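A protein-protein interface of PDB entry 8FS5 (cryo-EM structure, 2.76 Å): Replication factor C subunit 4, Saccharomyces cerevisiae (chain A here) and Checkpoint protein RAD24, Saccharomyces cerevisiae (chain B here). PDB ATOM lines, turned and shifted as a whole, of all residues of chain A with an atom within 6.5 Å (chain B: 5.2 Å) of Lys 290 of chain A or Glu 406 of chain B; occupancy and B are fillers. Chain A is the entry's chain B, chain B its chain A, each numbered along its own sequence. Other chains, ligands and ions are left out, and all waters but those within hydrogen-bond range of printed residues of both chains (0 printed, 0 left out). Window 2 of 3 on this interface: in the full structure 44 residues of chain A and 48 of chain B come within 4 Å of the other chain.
The side-chain carboxylate of Glu 406 of chain B is in salt-bridge range of the side-chain amino group of Lys 290 of chain A, 3.1 Å away.
Tyr 419 of chain B touches Leu 286 of chain A (CD1 to O, 3.1 Å).
Lys 290 of chain A touches Tyr 419 of chain B.
Of the printed residues of chain B, Leu 286 of chain A touches Tyr 419 (3.1 Å).
Of chain B, only Glu 406 (3.1 Å) and Tyr 419 (3.5 Å) come within 4 Å of Lys 290 of chain A.
Glu 406 of chain B touches just one residue of chain A: Lys 290.
Of the printed residues of chain A, Tyr 419 of chain B touches Leu 286 and Lys 290.
Hydrophobic or aromatic side chains of chain B that line the printed part of chain A: Tyr 419.
Of the 11 printed residues of chain A, 2 touch a printed residue of chain B.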
ATOM      1  N   ARG A 285      21.769   4.392  22.730  1.00  0.00           N
ATOM      2  CA  ARG A 285      22.889   5.135  23.299  1.00  0.00           C
ATOM      3  C   ARG A 285      23.689   4.291  24.283  1.00  0.00           C
ATOM      4  O   ARG A 285      24.925   4.319  24.270  1.00  0.00           O
ATOM      5  CB  ARG A 285      22.378   6.407  23.978  1.00  0.00           C
ATOM      6  CG  ARG A 285      23.466   7.240  24.636  1.00  0.00           C
ATOM      7  CD  ARG A 285      22.872   8.303  25.541  1.00  0.00           C
ATOM      8  NE  ARG A 285      21.689   8.918  24.952  1.00  0.00           N
ATOM      9  CZ  ARG A 285      21.715   9.955  24.128  1.00  0.00           C
ATOM     10  NH1 ARG A 285      22.855  10.524  23.769  1.00  0.00           N
ATOM     11  NH2 ARG A 285      20.570  10.436  23.651  1.00  0.00           N
ATOM     12  N   LEU A 286      23.007   3.537  25.148  1.00  0.00           N
ATOM     13  CA  LEU A 286      23.718   2.691  26.101  1.00  0.00           C
ATOM     14  C   LEU A 286      24.493   1.567  25.424  1.00  0.00           C
ATOM     15  O   LEU A 286      25.616   1.268  25.844  1.00  0.00           O
ATOM     16  CB  LEU A 286      22.747   2.125  27.144  1.00  0.00           C
ATOM     17  CG  LEU A 286      21.527   1.291  26.743  1.00  0.00           C
ATOM     18  CD1 LEU A 286      21.842  -0.196  26.673  1.00  0.00           C
ATOM     19  CD2 LEU A 286      20.386   1.547  27.716  1.00  0.00           C
ATOM     20  N   GLU A 287      23.933   0.950  24.382  1.00  0.00           N
ATOM     21  CA  GLU A 287      24.682  -0.052  23.631  1.00  0.00           C
ATOM     22  C   GLU A 287      25.886   0.551  22.921  1.00  0.00           C
ATOM     23  O   GLU A 287      26.952  -0.076  22.877  1.00  0.00           O
ATOM     24  CB  GLU A 287      23.766  -0.755  22.627  1.00  0.00           C
ATOM     25  CG  GLU A 287      22.607  -1.514  23.255  1.00  0.00           C
ATOM     26  CD  GLU A 287      23.053  -2.741  24.032  1.00  0.00           C
ATOM     27  OE1 GLU A 287      24.176  -3.231  23.791  1.00  0.00           O
ATOM     28  OE2 GLU A 287      22.275  -3.217  24.886  1.00  0.00           O
ATOM     29  N   MET A 288      25.744   1.760  22.367  1.00  0.00           N
ATOM     30  CA  MET A 288      26.892   2.439  21.775  1.00  0.00           C
ATOM     31  C   MET A 288      27.969   2.723  22.815  1.00  0.00           C
ATOM     32  O   MET A 288      29.161   2.554  22.538  1.00  0.00           O
ATOM     33  CB  MET A 288      26.452   3.737  21.097  1.00  0.00           C
ATOM     34  CG  MET A 288      25.626   3.539  19.840  1.00  0.00           C
ATOM     35  SD  MET A 288      24.959   5.086  19.197  1.00  0.00           S
ATOM     36  CE  MET A 288      26.467   5.955  18.775  1.00  0.00           C
ATOM     37  N   ILE A 289      27.563   3.152  24.013  1.00  0.00           N
ATOM     38  CA  ILE A 289      28.515   3.377  25.097  1.00  0.00           C
ATOM     39  C   ILE A 289      29.222   2.082  25.473  1.00  0.00           C
ATOM     40  O   ILE A 289      30.434   2.076  25.717  1.00  0.00           O
ATOM     41  CB  ILE A 289      27.803   4.012  26.310  1.00  0.00           C
ATOM     42  CG1 ILE A 289      27.384   5.448  25.991  1.00  0.00           C
ATOM     43  CG2 ILE A 289      28.691   3.981  27.545  1.00  0.00           C
ATOM     44  CD1 ILE A 289      26.683   6.150  27.132  1.00  0.00           C
ATOM     45  N   LYS A 290      28.487   0.970  25.523  1.00  0.00           N
ATOM     46  CA  LYS A 290      29.093  -0.325  25.825  1.00  0.00           C
ATOM     47  C   LYS A 290      30.119  -0.734  24.772  1.00  0.00           C
ATOM     48  O   LYS A 290      31.212  -1.205  25.116  1.00  0.00           O
ATOM     49  CB  LYS A 290      28.007  -1.393  25.947  1.00  0.00           C
ATOM     50  CG  LYS A 290      28.538  -2.792  26.200  1.00  0.00           C
ATOM     51  CD  LYS A 290      27.419  -3.818  26.158  1.00  0.00           C
ATOM     52  CE  LYS A 290      27.968  -5.229  26.052  1.00  0.00           C
ATOM     53  NZ  LYS A 290      26.882  -6.240  25.950  1.00  0.00           N
ATOM     54  N   GLU A 291      29.783  -0.572  23.489  1.00  0.00           N
ATOM     55  CA  GLU A 291      30.734  -0.915  22.434  1.00  0.00           C
ATOM     56  C   GLU A 291      31.964  -0.015  22.481  1.00  0.00           C
ATOM     57  O   GLU A 291      33.095  -0.488  22.299  1.00  0.00           O
ATOM     58  CB  GLU A 291      30.065  -0.838  21.061  1.00  0.00           C
ATOM     59  CG  GLU A 291      28.800  -1.678  20.912  1.00  0.00           C
ATOM     60  CD  GLU A 291      28.969  -3.113  21.384  1.00  0.00           C
ATOM     61  OE1 GLU A 291      30.033  -3.715  21.126  1.00  0.00           O
ATOM     62  OE2 GLU A 291      28.029  -3.640  22.015  1.00  0.00           O
ATOM     63  N   ILE A 292      31.766   1.282  22.731  1.00  0.00           N
ATOM     64  CA  ILE A 292      32.894   2.200  22.844  1.00  0.00           C
ATOM     65  C   ILE A 292      33.766   1.839  24.040  1.00  0.00           C
ATOM     66  O   ILE A 292      34.994   1.927  23.965  1.00  0.00           O
ATOM     67  CB  ILE A 292      32.390   3.655  22.913  1.00  0.00           C
ATOM     68  CG1 ILE A 292      31.789   4.070  21.569  1.00  0.00           C
ATOM     69  CG2 ILE A 292      33.510   4.610  23.299  1.00  0.00           C
ATOM     70  CD1 ILE A 292      30.953   5.325  21.635  1.00  0.00           C
ATOM     71  N   GLY A 293      33.160   1.409  25.150  1.00  0.00           N
ATOM     72  CA  GLY A 293      33.942   0.971  26.294  1.00  0.00           C
ATOM     73  C   GLY A 293      34.738  -0.292  26.046  1.00  0.00           C
ATOM     74  O   GLY A 293      35.889  -0.396  26.487  1.00  0.00           O
ATOM     75  N   LEU A 294      34.147  -1.268  25.354  1.00  0.00           N
ATOM     76  CA  LEU A 294      34.898  -2.465  24.985  1.00  0.00           C
ATOM     77  C   LEU A 294      36.059  -2.125  24.057  1.00  0.00           C
ATOM     78  O   LEU A 294      37.171  -2.649  24.219  1.00  0.00           O
ATOM     79  CB  LEU A 294      33.970  -3.489  24.332  1.00  0.00           C
ATOM     80  CG  LEU A 294      32.896  -4.097  25.236  1.00  0.00           C
ATOM     81  CD1 LEU A 294      31.970  -5.002  24.438  1.00  0.00           C
ATOM     82  CD2 LEU A 294      33.532  -4.857  26.391  1.00  0.00           C
ATOM     83  N   THR A 295      35.821  -1.236  23.089  1.00  0.00           N
ATOM     84  CA  THR A 295      36.899  -0.782  22.218  1.00  0.00           C
ATOM     85  C   THR A 295      37.973  -0.046  23.011  1.00  0.00           C
ATOM     86  O   THR A 295      39.166  -0.193  22.731  1.00  0.00           O
ATOM     87  CB  THR A 295      36.336   0.108  21.110  1.00  0.00           C
ATOM     88  OG1 THR A 295      35.318  -0.608  20.401  1.00  0.00           O
ATOM     89  CG2 THR A 295      37.430   0.509  20.132  1.00  0.00           C
ATOM     90  N   VAL B 401      21.293  -7.723  36.022  1.00  0.00           N
ATOM     91  CA  VAL B 401      22.452  -8.365  36.635  1.00  0.00           C
ATOM     92  C   VAL B 401      23.494  -8.753  35.586  1.00  0.00           C
ATOM     93  O   VAL B 401      24.698  -8.676  35.853  1.00  0.00           O
ATOM     94  CB  VAL B 401      22.025  -9.571  37.488  1.00  0.00           C
ATOM     95  CG1 VAL B 401      23.205 -10.087  38.284  1.00  0.00           C
ATOM     96  CG2 VAL B 401      20.919  -9.172  38.442  1.00  0.00           C
ATOM     97  N   ASP B 402      23.069  -9.166  34.388  1.00  0.00           N
ATOM     98  CA  ASP B 402      24.020  -9.442  33.317  1.00  0.00           C
ATOM     99  C   ASP B 402      24.768  -8.186  32.893  1.00  0.00           C
ATOM    100  O   ASP B 402      25.983  -8.241  32.664  1.00  0.00           O
ATOM    101  CB  ASP B 402      23.290 -10.074  32.126  1.00  0.00           C
ATOM    102  CG  ASP B 402      24.133 -10.110  30.859  1.00  0.00           C
ATOM    103  OD1 ASP B 402      24.244  -9.073  30.169  1.00  0.00           O
ATOM    104  OD2 ASP B 402      24.687 -11.185  30.552  1.00  0.00           O
ATOM    105  N   CYS B 403      24.070  -7.051  32.791  1.00  0.00           N
ATOM    106  CA  CYS B 403      24.742  -5.796  32.480  1.00  0.00           C
ATOM    107  C   CYS B 403      25.730  -5.404  33.569  1.00  0.00           C
ATOM    108  O   CYS B 403      26.833  -4.942  33.261  1.00  0.00           O
ATOM    109  CB  CYS B 403      23.716  -4.685  32.275  1.00  0.00           C
ATOM    110  SG  CYS B 403      24.399  -3.028  32.449  1.00  0.00           S
ATOM    111  N   LEU B 404      25.358  -5.577  34.839  1.00  0.00           N
ATOM    112  CA  LEU B 404      26.287  -5.302  35.931  1.00  0.00           C
ATOM    113  C   LEU B 404      27.510  -6.212  35.902  1.00  0.00           C
ATOM    114  O   LEU B 404      28.628  -5.738  36.139  1.00  0.00           O
ATOM    115  CB  LEU B 404      25.573  -5.434  37.279  1.00  0.00           C
ATOM    116  CG  LEU B 404      25.119  -4.139  37.959  1.00  0.00           C
ATOM    117  CD1 LEU B 404      24.481  -3.179  36.964  1.00  0.00           C
ATOM    118  CD2 LEU B 404      24.159  -4.443  39.098  1.00  0.00           C
ATOM    119  N   SER B 405      27.322  -7.501  35.611  1.00  0.00           N
ATOM    120  CA  SER B 405      28.455  -8.415  35.502  1.00  0.00           C
ATOM    121  C   SER B 405      29.366  -8.030  34.343  1.00  0.00           C
ATOM    122  O   SER B 405      30.595  -8.106  34.461  1.00  0.00           O
ATOM    123  CB  SER B 405      27.956  -9.851  35.338  1.00  0.00           C
ATOM    124  OG  SER B 405      27.333 -10.033  34.079  1.00  0.00           O
ATOM    125  N   GLU B 406      28.785  -7.619  33.213  1.00  0.00           N
ATOM    126  CA  GLU B 406      29.593  -7.159  32.089  1.00  0.00           C
ATOM    127  C   GLU B 406      30.333  -5.864  32.402  1.00  0.00           C
ATOM    128  O   GLU B 406      31.477  -5.699  31.964  1.00  0.00           O
ATOM    129  CB  GLU B 406      28.718  -6.977  30.849  1.00  0.00           C
ATOM    130  CG  GLU B 406      29.406  -7.362  29.551  1.00  0.00           C
ATOM    131  CD  GLU B 406      28.425  -7.757  28.465  1.00  0.00           C
ATOM    132  OE1 GLU B 406      27.204  -7.718  28.723  1.00  0.00           O
ATOM    133  OE2 GLU B 406      28.876  -8.108  27.354  1.00  0.00           O
ATOM    134  N   CYS B 407      29.709  -4.948  33.143  1.00  0.00           N
ATOM    135  CA  CYS B 407      30.373  -3.731  33.589  1.00  0.00           C
ATOM    136  C   CYS B 407      31.504  -4.002  34.567  1.00  0.00           C
ATOM    137  O   CYS B 407      32.498  -3.266  34.563  1.00  0.00           O
ATOM    138  CB  CYS B 407      29.365  -2.784  34.248  1.00  0.00           C
ATOM    139  SG  CYS B 407      28.146  -2.081  33.124  1.00  0.00           S
ATOM    140  N   ASP B 408      31.372  -5.032  35.402  1.00  0.00           N
ATOM    141  CA  ASP B 408      32.431  -5.407  36.331  1.00  0.00           C
ATOM    142  C   ASP B 408      33.708  -5.855  35.629  1.00  0.00           C
ATOM    143  O   ASP B 408      34.771  -5.871  36.260  1.00  0.00           O
ATOM    144  CB  ASP B 408      31.936  -6.518  37.262  1.00  0.00           C
ATOM    145  CG  ASP B 408      32.874  -6.767  38.426  1.00  0.00           C
ATOM    146  OD1 ASP B 408      33.262  -5.790  39.099  1.00  0.00           O
ATOM    147  OD2 ASP B 408      33.225  -7.941  38.667  1.00  0.00           O
ATOM    148  N   ASN B 409      33.635  -6.205  34.345  1.00  0.00           N
ATOM    149  CA  ASN B 409      34.789  -6.670  33.586  1.00  0.00           C
ATOM    150  C   ASN B 409      35.452  -5.561  32.779  1.00  0.00           C
ATOM    151  O   ASN B 409      36.349  -5.846  31.978  1.00  0.00           O
ATOM    152  CB  ASN B 409      34.380  -7.811  32.652  1.00  0.00           C
ATOM    153  CG  ASN B 409      34.021  -9.079  33.398  1.00  0.00           C
ATOM    154  OD1 ASN B 409      33.538 -10.040  32.805  1.00  0.00           O
ATOM    155  ND2 ASN B 409      34.265  -9.091  34.703  1.00  0.00           N
ATOM    156  N   MET B 410      35.038  -4.308  32.966  1.00  0.00           N
ATOM    157  CA  MET B 410      35.555  -3.189  32.187  1.00  0.00           C
ATOM    158  C   MET B 410      36.640  -2.420  32.936  1.00  0.00           C
ATOM    159  O   MET B 410      37.041  -1.333  32.509  1.00  0.00           O
ATOM    160  CB  MET B 410      34.418  -2.256  31.775  1.00  0.00           C
ATOM    161  CG  MET B 410      33.581  -2.786  30.621  1.00  0.00           C
ATOM    162  SD  MET B 410      33.001  -1.491  29.510  1.00  0.00           S
ATOM    163  CE  MET B 410      31.244  -1.837  29.475  1.00  0.00           C
ATOM    164  N   TYR B 419      27.251   2.977  31.359  1.00  0.00           N
ATOM    165  CA  TYR B 419      26.437   1.957  30.711  1.00  0.00           C
ATOM    166  C   TYR B 419      25.567   1.193  31.696  1.00  0.00           C
ATOM    167  O   TYR B 419      24.397   0.929  31.404  1.00  0.00           O
ATOM    168  CB  TYR B 419      27.325   0.974  29.941  1.00  0.00           C
ATOM    169  CG  TYR B 419      26.602  -0.274  29.479  1.00  0.00           C
ATOM    170  CD1 TYR B 419      25.543  -0.198  28.586  1.00  0.00           C
ATOM    171  CD2 TYR B 419      26.988  -1.528  29.930  1.00  0.00           C
ATOM    172  CE1 TYR B 419      24.883  -1.336  28.162  1.00  0.00           C
ATOM    173  CE2 TYR B 419      26.334  -2.672  29.513  1.00  0.00           C
ATOM    174  CZ  TYR B 419      25.282  -2.569  28.629  1.00  0.00           C
ATOM    175  OH  TYR B 419      24.629  -3.705  28.209  1.00  0.00           O
